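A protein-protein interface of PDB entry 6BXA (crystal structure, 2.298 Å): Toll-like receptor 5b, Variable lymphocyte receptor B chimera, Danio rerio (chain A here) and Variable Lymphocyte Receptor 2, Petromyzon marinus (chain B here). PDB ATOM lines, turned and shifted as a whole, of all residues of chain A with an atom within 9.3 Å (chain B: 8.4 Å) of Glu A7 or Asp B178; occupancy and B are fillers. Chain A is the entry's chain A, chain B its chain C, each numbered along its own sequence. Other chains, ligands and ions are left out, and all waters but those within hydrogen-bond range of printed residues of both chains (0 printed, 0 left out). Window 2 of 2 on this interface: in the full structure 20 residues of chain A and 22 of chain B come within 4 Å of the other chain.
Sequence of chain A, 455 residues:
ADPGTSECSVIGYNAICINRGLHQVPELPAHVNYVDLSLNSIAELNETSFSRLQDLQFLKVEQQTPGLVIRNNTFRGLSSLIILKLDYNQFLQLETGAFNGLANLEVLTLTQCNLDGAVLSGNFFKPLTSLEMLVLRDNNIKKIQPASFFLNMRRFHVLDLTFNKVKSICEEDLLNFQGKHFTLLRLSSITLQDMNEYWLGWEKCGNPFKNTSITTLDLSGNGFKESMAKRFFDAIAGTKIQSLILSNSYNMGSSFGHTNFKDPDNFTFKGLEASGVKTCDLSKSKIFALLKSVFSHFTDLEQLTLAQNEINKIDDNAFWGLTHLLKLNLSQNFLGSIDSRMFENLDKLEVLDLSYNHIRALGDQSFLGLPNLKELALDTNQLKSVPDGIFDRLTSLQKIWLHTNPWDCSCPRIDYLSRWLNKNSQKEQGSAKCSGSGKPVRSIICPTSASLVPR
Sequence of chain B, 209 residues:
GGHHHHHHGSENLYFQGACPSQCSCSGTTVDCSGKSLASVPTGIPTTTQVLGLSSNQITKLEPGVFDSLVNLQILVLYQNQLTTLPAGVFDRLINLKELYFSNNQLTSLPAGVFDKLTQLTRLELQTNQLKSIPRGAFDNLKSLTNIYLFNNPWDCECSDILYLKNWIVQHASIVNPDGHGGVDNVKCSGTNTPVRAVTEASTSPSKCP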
ATOM      1  N   GLU A   7       2.009  -8.008  -4.705  1.00  0.00           N
ATOM      2  CA  GLU A   7       3.384  -8.492  -4.747  1.00  0.00           C
ATOM      3  C   GLU A   7       3.622  -9.498  -5.878  1.00  0.00           C
ATOM      4  O   GLU A   7       4.771  -9.757  -6.251  1.00  0.00           O
ATOM      5  CB  GLU A   7       3.751  -9.112  -3.399  1.00  0.00           C
ATOM      6  CG  GLU A   7       5.223  -9.036  -3.056  1.00  0.00           C
ATOM      7  CD  GLU A   7       5.517  -9.593  -1.683  1.00  0.00           C
ATOM      8  OE1 GLU A   7       4.659  -9.454  -0.782  1.00  0.00           O
ATOM      9  OE2 GLU A   7       6.587 -10.209  -1.515  1.00  0.00           O
ATOM     10  N   CYS A   8       2.550 -10.066  -6.422  1.00  0.00           N
ATOM     11  CA  CYS A   8       2.681 -10.953  -7.578  1.00  0.00           C
ATOM     12  C   CYS A   8       3.104 -10.155  -8.810  1.00  0.00           C
ATOM     13  O   CYS A   8       2.787  -8.982  -8.946  1.00  0.00           O
ATOM     14  CB  CYS A   8       1.371 -11.696  -7.872  1.00  0.00           C
ATOM     15  SG  CYS A   8       0.903 -12.992  -6.701  1.00  0.00           S
ATOM     16  N   SER A   9       3.802 -10.818  -9.716  1.00  0.00           N
ATOM     17  CA  SER A   9       4.159 -10.238 -10.994  1.00  0.00           C
ATOM     18  C   SER A   9       3.106 -10.620 -12.036  1.00  0.00           C
ATOM     19  O   SER A   9       2.952 -11.796 -12.370  1.00  0.00           O
ATOM     20  CB  SER A   9       5.549 -10.715 -11.415  1.00  0.00           C
ATOM     21  OG  SER A   9       5.689 -10.711 -12.821  1.00  0.00           O
ATOM     22  N   VAL A  10       2.358  -9.632 -12.518  1.00  0.00           N
ATOM     23  CA  VAL A  10       1.327  -9.871 -13.521  1.00  0.00           C
ATOM     24  C   VAL A  10       1.791  -9.472 -14.920  1.00  0.00           C
ATOM     25  O   VAL A  10       2.163  -8.329 -15.166  1.00  0.00           O
ATOM     26  CB  VAL A  10       0.019  -9.117 -13.184  1.00  0.00           C
ATOM     27  CG1 VAL A  10      -0.956  -9.201 -14.335  1.00  0.00           C
ATOM     28  CG2 VAL A  10      -0.604  -9.666 -11.915  1.00  0.00           C
ATOM     29  N   ALA A  15      -0.039 -14.709 -13.985  1.00  0.00           N
ATOM     30  CA  ALA A  15       0.275 -14.167 -12.668  1.00  0.00           C
ATOM     31  C   ALA A  15       1.309 -15.042 -11.985  1.00  0.00           C
ATOM     32  O   ALA A  15       1.056 -16.213 -11.693  1.00  0.00           O
ATOM     33  CB  ALA A  15      -0.976 -14.053 -11.814  1.00  0.00           C
ATOM     34  N   ILE A  16       2.480 -14.473 -11.739  1.00  0.00           N
ATOM     35  CA  ILE A  16       3.557 -15.211 -11.096  1.00  0.00           C
ATOM     36  C   ILE A  16       3.677 -14.804  -9.638  1.00  0.00           C
ATOM     37  O   ILE A  16       4.031 -13.667  -9.320  1.00  0.00           O
ATOM     38  CB  ILE A  16       4.888 -14.978 -11.812  1.00  0.00           C
ATOM     39  CG1 ILE A  16       4.715 -15.255 -13.307  1.00  0.00           C
ATOM     40  CG2 ILE A  16       5.986 -15.835 -11.208  1.00  0.00           C
ATOM     41  CD1 ILE A  16       4.235 -16.639 -13.636  1.00  0.00           C
ATOM     42  N   CYS A  17       3.384 -15.748  -8.752  1.00  0.00           N
ATOM     43  CA  CYS A  17       3.388 -15.474  -7.329  1.00  0.00           C
ATOM     44  C   CYS A  17       4.325 -16.403  -6.587  1.00  0.00           C
ATOM     45  O   CYS A  17       4.103 -16.697  -5.418  1.00  0.00           O
ATOM     46  CB  CYS A  17       1.980 -15.614  -6.770  1.00  0.00           C
ATOM     47  SG  CYS A  17       0.747 -14.757  -7.750  1.00  0.00           S
ATOM     48  N   ILE A  18       5.370 -16.854  -7.273  1.00  0.00           N
ATOM     49  CA  ILE A  18       6.355 -17.766  -6.698  1.00  0.00           C
ATOM     50  C   ILE A  18       7.107 -17.127  -5.541  1.00  0.00           C
ATOM     51  O   ILE A  18       7.645 -16.032  -5.678  1.00  0.00           O
ATOM     52  CB  ILE A  18       7.392 -18.219  -7.759  1.00  0.00           C
ATOM     53  CG1 ILE A  18       6.693 -18.823  -8.981  1.00  0.00           C
ATOM     54  CG2 ILE A  18       8.391 -19.201  -7.161  1.00  0.00           C
ATOM     55  CD1 ILE A  18       7.626 -19.077 -10.154  1.00  0.00           C
ATOM     56  N   ASN A  19       7.135 -17.809  -4.402  1.00  0.00           N
ATOM     57  CA  ASN A  19       7.958 -17.392  -3.277  1.00  0.00           C
ATOM     58  C   ASN A  19       7.702 -15.945  -2.872  1.00  0.00           C
ATOM     59  O   ASN A  19       8.580 -15.081  -2.986  1.00  0.00           O
ATOM     60  CB  ASN A  19       9.437 -17.583  -3.604  1.00  0.00           C
ATOM     61  CG  ASN A  19      10.322 -17.355  -2.403  1.00  0.00           C
ATOM     62  OD1 ASN A  19       9.989 -17.765  -1.295  1.00  0.00           O
ATOM     63  ND2 ASN A  19      11.430 -16.653  -2.606  1.00  0.00           N
ATOM     64  N   ARG A  20       6.480 -15.679  -2.442  1.00  0.00           N
ATOM     65  CA  ARG A  20       6.088 -14.339  -2.040  1.00  0.00           C
ATOM     66  C   ARG A  20       5.729 -14.310  -0.560  1.00  0.00           C
ATOM     67  O   ARG A  20       5.276 -13.294  -0.047  1.00  0.00           O
ATOM     68  CB  ARG A  20       4.910 -13.847  -2.883  1.00  0.00           C
ATOM     69  CG  ARG A  20       5.282 -12.795  -3.899  1.00  0.00           C
ATOM     70  CD  ARG A  20       6.070 -13.389  -5.035  1.00  0.00           C
ATOM     71  NE  ARG A  20       6.228 -12.444  -6.135  1.00  0.00           N
ATOM     72  CZ  ARG A  20       6.927 -12.703  -7.233  1.00  0.00           C
ATOM     73  NH1 ARG A  20       7.531 -13.880  -7.379  1.00  0.00           N
ATOM     74  NH2 ARG A  20       7.020 -11.793  -8.188  1.00  0.00           N
ATOM     75  N   GLY A  21       5.920 -15.435   0.121  1.00  0.00           N
ATOM     76  CA  GLY A  21       5.602 -15.524   1.535  1.00  0.00           C
ATOM     77  C   GLY A  21       4.110 -15.429   1.800  1.00  0.00           C
ATOM     78  O   GLY A  21       3.691 -15.016   2.872  1.00  0.00           O
ATOM     79  N   LEU A  22       3.313 -15.834   0.820  1.00  0.00           N
ATOM     80  CA  LEU A  22       1.859 -15.722   0.896  1.00  0.00           C
ATOM     81  C   LEU A  22       1.251 -16.788   1.800  1.00  0.00           C
ATOM     82  O   LEU A  22       1.696 -17.938   1.810  1.00  0.00           O
ATOM     83  CB  LEU A  22       1.253 -15.820  -0.508  1.00  0.00           C
ATOM     84  CG  LEU A  22       1.736 -14.732  -1.476  1.00  0.00           C
ATOM     85  CD1 LEU A  22       1.231 -14.965  -2.893  1.00  0.00           C
ATOM     86  CD2 LEU A  22       1.347 -13.342  -0.974  1.00  0.00           C
ATOM     87  N   HIS A  23       0.229 -16.400   2.556  1.00  0.00           N
ATOM     88  CA  HIS A  23      -0.477 -17.308   3.457  1.00  0.00           C
ATOM     89  C   HIS A  23      -1.891 -17.556   2.968  1.00  0.00           C
ATOM     90  O   HIS A  23      -2.635 -18.348   3.550  1.00  0.00           O
ATOM     91  CB  HIS A  23      -0.503 -16.741   4.878  1.00  0.00           C
ATOM     92  CG  HIS A  23       0.835 -16.743   5.534  1.00  0.00           C
ATOM     93  ND1 HIS A  23       1.297 -17.810   6.272  1.00  0.00           N
ATOM     94  CD2 HIS A  23       1.831 -15.829   5.527  1.00  0.00           C
ATOM     95  CE1 HIS A  23       2.517 -17.549   6.706  1.00  0.00           C
ATOM     96  NE2 HIS A  23       2.863 -16.351   6.268  1.00  0.00           N
ATOM     97  N   PRO A  26      -3.746 -14.254  -3.084  1.00  0.00           N
ATOM     98  CA  PRO A  26      -3.771 -12.790  -3.182  1.00  0.00           C
ATOM     99  C   PRO A  26      -4.793 -12.249  -4.182  1.00  0.00           C
ATOM    100  O   PRO A  26      -5.336 -12.994  -4.997  1.00  0.00           O
ATOM    101  CB  PRO A  26      -2.353 -12.455  -3.639  1.00  0.00           C
ATOM    102  CG  PRO A  26      -1.950 -13.631  -4.450  1.00  0.00           C
ATOM    103  CD  PRO A  26      -2.569 -14.827  -3.761  1.00  0.00           C
ATOM    104  N   GLU A  27      -5.058 -10.951  -4.102  1.00  0.00           N
ATOM    105  CA  GLU A  27      -5.927 -10.297  -5.071  1.00  0.00           C
ATOM    106  C   GLU A  27      -5.211 -10.188  -6.419  1.00  0.00           C
ATOM    107  O   GLU A  27      -4.079  -9.706  -6.512  1.00  0.00           O
ATOM    108  CB  GLU A  27      -6.359  -8.917  -4.572  1.00  0.00           C
ATOM    109  N   LEU A  28      -5.876 -10.662  -7.463  1.00  0.00           N
ATOM    110  CA  LEU A  28      -5.320 -10.631  -8.806  1.00  0.00           C
ATOM    111  C   LEU A  28      -6.373 -10.135  -9.778  1.00  0.00           C
ATOM    112  O   LEU A  28      -7.568 -10.237  -9.497  1.00  0.00           O
ATOM    113  CB  LEU A  28      -4.818 -12.021  -9.222  1.00  0.00           C
ATOM    114  CG  LEU A  28      -3.620 -12.617  -8.474  1.00  0.00           C
ATOM    115  CD1 LEU A  28      -3.401 -14.088  -8.851  1.00  0.00           C
ATOM    116  CD2 LEU A  28      -2.365 -11.788  -8.750  1.00  0.00           C
ATOM    117  N   ASP A  36       0.695 -19.052 -10.961  1.00  0.00           N
ATOM    118  CA  ASP A  36       1.654 -19.888 -10.258  1.00  0.00           C
ATOM    119  C   ASP A  36       1.820 -19.410  -8.824  1.00  0.00           C
ATOM    120  O   ASP A  36       2.403 -18.350  -8.589  1.00  0.00           O
ATOM    121  CB  ASP A  36       3.004 -19.878 -10.969  1.00  0.00           C
ATOM    122  CG  ASP A  36       3.955 -20.939 -10.439  1.00  0.00           C
ATOM    123  OD1 ASP A  36       3.660 -21.548  -9.386  1.00  0.00           O
ATOM    124  OD2 ASP A  36       5.006 -21.160 -11.081  1.00  0.00           O
ATOM    125  N   LEU A  37       1.327 -20.209  -7.875  1.00  0.00           N
ATOM    126  CA  LEU A  37       1.404 -19.880  -6.453  1.00  0.00           C
ATOM    127  C   LEU A  37       2.400 -20.776  -5.710  1.00  0.00           C
ATOM    128  O   LEU A  37       2.341 -20.893  -4.485  1.00  0.00           O
ATOM    129  CB  LEU A  37       0.020 -19.993  -5.811  1.00  0.00           C
ATOM    130  CG  LEU A  37      -0.962 -18.862  -6.143  1.00  0.00           C
ATOM    131  CD1 LEU A  37      -2.374 -19.302  -5.850  1.00  0.00           C
ATOM    132  CD2 LEU A  37      -0.641 -17.613  -5.360  1.00  0.00           C
ATOM    133  N   ASN A  40       4.961 -21.081  -1.487  1.00  0.00           N
ATOM    134  CA  ASN A  40       4.452 -20.128  -0.516  1.00  0.00           C
ATOM    135  C   ASN A  40       4.039 -20.869   0.747  1.00  0.00           C
ATOM    136  O   ASN A  40       4.330 -22.053   0.898  1.00  0.00           O
ATOM    137  CB  ASN A  40       3.280 -19.315  -1.086  1.00  0.00           C
ATOM    138  CG  ASN A  40       3.737 -18.258  -2.078  1.00  0.00           C
ATOM    139  OD1 ASN A  40       4.219 -17.193  -1.687  1.00  0.00           O
ATOM    140  ND2 ASN A  40       3.610 -18.553  -3.364  1.00  0.00           N
ATOM    141  N   SER A  41       3.375 -20.167   1.659  1.00  0.00           N
ATOM    142  CA  SER A  41       3.024 -20.744   2.949  1.00  0.00           C
ATOM    143  C   SER A  41       1.520 -20.851   3.127  1.00  0.00           C
ATOM    144  O   SER A  41       1.002 -20.644   4.220  1.00  0.00           O
ATOM    145  CB  SER A  41       3.627 -19.908   4.076  1.00  0.00           C
ATOM    146  OG  SER A  41       5.033 -19.842   3.945  1.00  0.00           O
ATOM    147  N   GLU B  98      12.118 -11.368 -14.202  1.00  0.00           N
ATOM    148  CA  GLU B  98      12.315 -12.256 -13.049  1.00  0.00           C
ATOM    149  C   GLU B  98      13.145 -13.494 -13.387  1.00  0.00           C
ATOM    150  O   GLU B  98      12.885 -14.188 -14.379  1.00  0.00           O
ATOM    151  CB  GLU B  98      10.968 -12.697 -12.480  1.00  0.00           C
ATOM    152  CG  GLU B  98      10.188 -11.593 -11.815  1.00  0.00           C
ATOM    153  CD  GLU B  98       9.036 -12.110 -10.981  1.00  0.00           C
ATOM    154  OE1 GLU B  98       8.672 -13.298 -11.123  1.00  0.00           O
ATOM    155  OE2 GLU B  98       8.486 -11.318 -10.187  1.00  0.00           O
ATOM    156  N   TYR B 100      14.874 -16.994 -11.567  1.00  0.00           N
ATOM    157  CA  TYR B 100      14.868 -17.879 -10.400  1.00  0.00           C
ATOM    158  C   TYR B 100      15.923 -18.989 -10.475  1.00  0.00           C
ATOM    159  O   TYR B 100      15.834 -19.880 -11.323  1.00  0.00           O
ATOM    160  CB  TYR B 100      13.494 -18.526 -10.236  1.00  0.00           C
ATOM    161  CG  TYR B 100      12.341 -17.570 -10.021  1.00  0.00           C
ATOM    162  CD1 TYR B 100      11.682 -16.983 -11.100  1.00  0.00           C
ATOM    163  CD2 TYR B 100      11.882 -17.284  -8.744  1.00  0.00           C
ATOM    164  CE1 TYR B 100      10.613 -16.123 -10.907  1.00  0.00           C
ATOM    165  CE2 TYR B 100      10.814 -16.426  -8.541  1.00  0.00           C
ATOM    166  CZ  TYR B 100      10.184 -15.850  -9.620  1.00  0.00           C
ATOM    167  OH  TYR B 100       9.129 -14.997  -9.402  1.00  0.00           O
ATOM    168  N   THR B 121      13.774  -7.110 -12.054  1.00  0.00           N
ATOM    169  CA  THR B 121      13.353  -6.688 -10.724  1.00  0.00           C
ATOM    170  C   THR B 121      13.593  -7.770  -9.680  1.00  0.00           C
ATOM    171  O   THR B 121      13.873  -7.465  -8.522  1.00  0.00           O
ATOM    172  CB  THR B 121      11.866  -6.304 -10.685  1.00  0.00           C
ATOM    173  OG1 THR B 121      11.060  -7.458 -10.944  1.00  0.00           O
ATOM    174  CG2 THR B 121      11.563  -5.206 -11.700  1.00  0.00           C
ATOM    175  N   ARG B 122      13.491  -9.036 -10.076  1.00  0.00           N
ATOM    176  CA  ARG B 122      13.698 -10.128  -9.120  1.00  0.00           C
ATOM    177  C   ARG B 122      14.794 -11.100  -9.562  1.00  0.00           C
ATOM    178  O   ARG B 122      14.708 -11.726 -10.628  1.00  0.00           O
ATOM    179  CB  ARG B 122      12.394 -10.896  -8.888  1.00  0.00           C
ATOM    180  CG  ARG B 122      12.537 -12.030  -7.864  1.00  0.00           C
ATOM    181  CD  ARG B 122      11.236 -12.810  -7.696  1.00  0.00           C
ATOM    182  NE  ARG B 122      10.329 -12.173  -6.751  1.00  0.00           N
ATOM    183  CZ  ARG B 122      10.101 -12.610  -5.518  1.00  0.00           C
ATOM    184  NH1 ARG B 122      10.694 -13.712  -5.076  1.00  0.00           N
ATOM    185  NH2 ARG B 122       9.261 -11.950  -4.733  1.00  0.00           N
ATOM    186  N   THR B 145      14.459  -4.978  -7.553  1.00  0.00           N
ATOM    187  CA  THR B 145      13.606  -4.770  -6.391  1.00  0.00           C
ATOM    188  C   THR B 145      13.820  -5.849  -5.339  1.00  0.00           C
ATOM    189  O   THR B 145      13.802  -5.580  -4.142  1.00  0.00           O
ATOM    190  CB  THR B 145      12.123  -4.752  -6.807  1.00  0.00           C
ATOM    191  OG1 THR B 145      11.894  -3.629  -7.665  1.00  0.00           O
ATOM    192  CG2 THR B 145      11.213  -4.645  -5.591  1.00  0.00           C
ATOM    193  N   ASN B 146      14.034  -7.074  -5.800  1.00  0.00           N
ATOM    194  CA  ASN B 146      14.203  -8.211  -4.901  1.00  0.00           C
ATOM    195  C   ASN B 146      15.378  -9.086  -5.301  1.00  0.00           C
ATOM    196  O   ASN B 146      15.405  -9.638  -6.399  1.00  0.00           O
ATOM    197  CB  ASN B 146      12.929  -9.059  -4.857  1.00  0.00           C
ATOM    198  CG  ASN B 146      11.705  -8.258  -4.474  1.00  0.00           C
ATOM    199  OD1 ASN B 146      11.733  -7.474  -3.530  1.00  0.00           O
ATOM    200  ND2 ASN B 146      10.624  -8.445  -5.214  1.00  0.00           N
ATOM    201  N   ILE B 147      16.343  -9.222  -4.404  1.00  0.00           N
ATOM    202  CA  ILE B 147      17.425 -10.159  -4.619  1.00  0.00           C
ATOM    203  C   ILE B 147      17.570 -11.027  -3.379  1.00  0.00           C
ATOM    204  O   ILE B 147      17.482 -10.542  -2.246  1.00  0.00           O
ATOM    205  CB  ILE B 147      18.769  -9.453  -4.957  1.00  0.00           C
ATOM    206  CG1 ILE B 147      19.832 -10.484  -5.350  1.00  0.00           C
ATOM    207  CG2 ILE B 147      19.258  -8.607  -3.798  1.00  0.00           C
ATOM    208  CD1 ILE B 147      21.137  -9.880  -5.835  1.00  0.00           C
ATOM    209  N   TYR B 148      17.741 -12.323  -3.605  1.00  0.00           N
ATOM    210  CA  TYR B 148      17.878 -13.283  -2.514  1.00  0.00           C
ATOM    211  C   TYR B 148      19.233 -13.956  -2.633  1.00  0.00           C
ATOM    212  O   TYR B 148      19.582 -14.495  -3.687  1.00  0.00           O
ATOM    213  CB  TYR B 148      16.741 -14.307  -2.525  1.00  0.00           C
ATOM    214  CG  TYR B 148      15.368 -13.675  -2.461  1.00  0.00           C
ATOM    215  CD1 TYR B 148      14.734 -13.228  -3.612  1.00  0.00           C
ATOM    216  CD2 TYR B 148      14.720 -13.499  -1.247  1.00  0.00           C
ATOM    217  CE1 TYR B 148      13.482 -12.638  -3.560  1.00  0.00           C
ATOM    218  CE2 TYR B 148      13.465 -12.908  -1.184  1.00  0.00           C
ATOM    219  CZ  TYR B 148      12.852 -12.482  -2.342  1.00  0.00           C
ATOM    220  OH  TYR B 148      11.609 -11.894  -2.285  1.00  0.00           O
ATOM    221  N   SER B 173      18.105  -2.605   1.403  1.00  0.00           N
ATOM    222  CA  SER B 173      16.645  -2.637   1.444  1.00  0.00           C
ATOM    223  C   SER B 173      16.064  -3.673   0.488  1.00  0.00           C
ATOM    224  O   SER B 173      14.982  -4.202   0.736  1.00  0.00           O
ATOM    225  CB  SER B 173      16.061  -1.255   1.131  1.00  0.00           C
ATOM    226  OG  SER B 173      16.544  -0.744  -0.103  1.00  0.00           O
ATOM    227  N   ILE B 174      16.775  -3.967  -0.600  1.00  0.00           N
ATOM    228  CA  ILE B 174      16.301  -4.957  -1.568  1.00  0.00           C
ATOM    229  C   ILE B 174      16.914  -6.339  -1.351  1.00  0.00           C
ATOM    230  O   ILE B 174      16.640  -7.262  -2.116  1.00  0.00           O
ATOM    231  CB  ILE B 174      16.577  -4.528  -3.027  1.00  0.00           C
ATOM    232  CG1 ILE B 174      18.078  -4.447  -3.293  1.00  0.00           C
ATOM    233  CG2 ILE B 174      15.902  -3.203  -3.334  1.00  0.00           C
ATOM    234  CD1 ILE B 174      18.421  -4.297  -4.745  1.00  0.00           C
ATOM    235  N   VAL B 175      17.756  -6.483  -0.332  1.00  0.00           N
ATOM    236  CA  VAL B 175      18.388  -7.777  -0.066  1.00  0.00           C
ATOM    237  C   VAL B 175      17.586  -8.611   0.937  1.00  0.00           C
ATOM    238  O   VAL B 175      17.318  -8.169   2.056  1.00  0.00           O
ATOM    239  CB  VAL B 175      19.827  -7.627   0.464  1.00  0.00           C
ATOM    240  CG1 VAL B 175      20.389  -8.996   0.851  1.00  0.00           C
ATOM    241  CG2 VAL B 175      20.714  -6.955  -0.574  1.00  0.00           C
ATOM    242  N   ASN B 176      17.214  -9.816   0.512  1.00  0.00           N
ATOM    243  CA  ASN B 176      16.429 -10.760   1.310  1.00  0.00           C
ATOM    244  C   ASN B 176      15.218 -10.136   1.994  1.00  0.00           C
ATOM    245  O   ASN B 176      15.086 -10.236   3.211  1.00  0.00           O
ATOM    246  CB  ASN B 176      17.306 -11.410   2.380  1.00  0.00           C
ATOM    247  CG  ASN B 176      18.517 -12.121   1.804  1.00  0.00           C
ATOM    248  OD1 ASN B 176      18.484 -12.642   0.684  1.00  0.00           O
ATOM    249  ND2 ASN B 176      19.601 -12.141   2.572  1.00  0.00           N
ATOM    250  N   PRO B 177      14.318  -9.511   1.219  1.00  0.00           N
ATOM    251  CA  PRO B 177      13.179  -8.858   1.865  1.00  0.00           C
ATOM    252  C   PRO B 177      12.060  -9.833   2.207  1.00  0.00           C
ATOM    253  O   PRO B 177      12.218 -11.036   2.006  1.00  0.00           O
ATOM    254  CB  PRO B 177      12.719  -7.847   0.813  1.00  0.00           C
ATOM    255  CG  PRO B 177      13.259  -8.365  -0.511  1.00  0.00           C
ATOM    256  CD  PRO B 177      14.188  -9.511  -0.246  1.00  0.00           C
ATOM    257  N   ASP B 178      10.947  -9.303   2.710  1.00  0.00           N
ATOM    258  CA  ASP B 178       9.769 -10.103   3.046  1.00  0.00           C
ATOM    259  C   ASP B 178      10.094 -11.193   4.064  1.00  0.00           C
ATOM    260  O   ASP B 178       9.676 -12.342   3.913  1.00  0.00           O
ATOM    261  CB  ASP B 178       9.158 -10.717   1.787  1.00  0.00           C
ATOM    262  CG  ASP B 178       9.049  -9.720   0.650  1.00  0.00           C
ATOM    263  OD1 ASP B 178       8.822  -8.520   0.920  1.00  0.00           O
ATOM    264  OD2 ASP B 178       9.212 -10.134  -0.517  1.00  0.00           O
ATOM    265  N   GLY B 179      10.849 -10.823   5.094  1.00  0.00           N
ATOM    266  CA  GLY B 179      11.187 -11.736   6.171  1.00  0.00           C
ATOM    267  C   GLY B 179      12.138 -12.862   5.812  1.00  0.00           C
ATOM    268  O   GLY B 179      12.058 -13.955   6.373  1.00  0.00           O
ATOM    269  N   HIS B 180      13.049 -12.599   4.880  1.00  0.00           N
ATOM    270  CA  HIS B 180      14.080 -13.573   4.541  1.00  0.00           C
ATOM    271  C   HIS B 180      15.398 -13.221   5.212  1.00  0.00           C
ATOM    272  O   HIS B 180      16.464 -13.619   4.737  1.00  0.00           O
ATOM    273  CB  HIS B 180      14.284 -13.668   3.031  1.00  0.00           C
ATOM    274  CG  HIS B 180      13.271 -14.522   2.332  1.00  0.00           C
ATOM    275  ND1 HIS B 180      12.049 -14.039   1.915  1.00  0.00           N
ATOM    276  CD2 HIS B 180      13.306 -15.826   1.967  1.00  0.00           C
ATOM    277  CE1 HIS B 180      11.376 -15.009   1.322  1.00  0.00           C
ATOM    278  NE2 HIS B 180      12.117 -16.103   1.339  1.00  0.00           N
ATOM    279  N   GLY B 181      15.321 -12.445   6.293  1.00  0.00           N
ATOM    280  CA  GLY B 181      16.483 -12.150   7.109  1.00  0.00           C
ATOM    281  C   GLY B 181      17.079 -10.779   6.868  1.00  0.00           C
ATOM    282  O   GLY B 181      17.773 -10.228   7.724  1.00  0.00           O
ATOM    283  N   GLY B 182      16.820 -10.226   5.693  1.00  0.00           N
ATOM    284  CA  GLY B 182      17.372  -8.932   5.344  1.00  0.00           C
ATOM    285  C   GLY B 182      18.825  -9.051   4.931  1.00  0.00           C
ATOM    286  O   GLY B 182      19.296 -10.137   4.591  1.00  0.00           O
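O of Asn A19 sits at hydrogen-bond distance from NH1 of Arg B122 (3.3 Å).
OE2 of Glu B98 is in salt-bridge range of NH2 of Arg A20, at 2.5 Å.
The guanidinium group (NH1) of Arg A20 is in hydrogen-bond range of the side-chain hydroxyl (OH) of Tyr B100 (2.8 Å).
The side-chain carboxylate (OD2) of Asp B178 sits close to the side-chain carboxylate (OE2) of Glu A7 (2.8 Å).
The guanidinium group of Arg A20 sits close to the guanidinium group of Arg B122, at 3.3 Å.
The backbone carbonyl oxygen of Ser A9 sits at hydrogen-bond distance from the backbone NH of Ile A16, at 2.8 Å.
The backbone carbonyl oxygen (O) of Ile A18 lies within hydrogen-bond range of the guanidinium group (NH1) of Arg A20 (2.7 Å).
OD1 of Asn A40 is in hydrogen-bond range of N of Arg A20 (2.8 Å).
OE2 of Glu B98 lies within salt-bridge range of NE of Arg B122 (3.99 Å).
The side-chain hydroxyl (OH) of Tyr B148 lies within hydrogen-bond range of the guanidinium group (NH2) of Arg B122 (3.4 Å).
The side-chain sulfur of Cys A8 forms a disulfide with the side-chain sulfur of Cys A17 (2.1 Å).
Among the printed residues, merely in contact across the chains: Ser A9 with Glu B98, Ile A16 with Glu B98, Ile A16 with Tyr B100, Asn A19 with His B180, Ile A18 with Arg B122 and Ile A18 with Tyr B100.
No residue of chain A comes within 4 Å of Pro B177.
No residue of chain A comes within 4 Å of Gly B179.
Of the printed residues of chain A, Tyr B100 touches Ile A16, Ile A18 and Arg A20.
Printed residues of chain B within 4 Å of Arg A20: Glu B98 (2.5 Å), Tyr B100 (2.8 Å) and Arg B122 (3.3 Å).
Of the printed residues of chain A, His B180 touches Asn A19 (3.8 Å).
Of the printed residues of chain A, Arg B122 touches Ile A18 (3.9 Å), Asn A19 (3.3 Å) and Arg A20 (3.3 Å).
Asn B176 touches none of the printed residues of chain A.
Gly A21 touches none of the printed residues of chain B.
The nearest residue of chain B that does not touch Glu A7 is Arg B122 (4.5 Å).
The nearest residue of chain A that does not touch Asp B178 is Arg A20 (5.0 Å).
Of the 20 printed residues of chain A, 6 touch a printed residue of chain B.
Hydrophobic or aromatic side chains of chain A that line the printed part of chain B: Ile A16 and Ile A18.
Printed residues of chain B that touch a printed residue of chain A: Glu B98, Tyr B100, Arg B122, Asp B178 and His B180.
Among the printed residues, 11 pairs touch across the chains.
Among the printed residues, Asp or Glu carboxylates within 4 Å of a Lys or Arg side-chain nitrogen of the other chain: Arg A20 with Glu B98 (2.5 Å).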
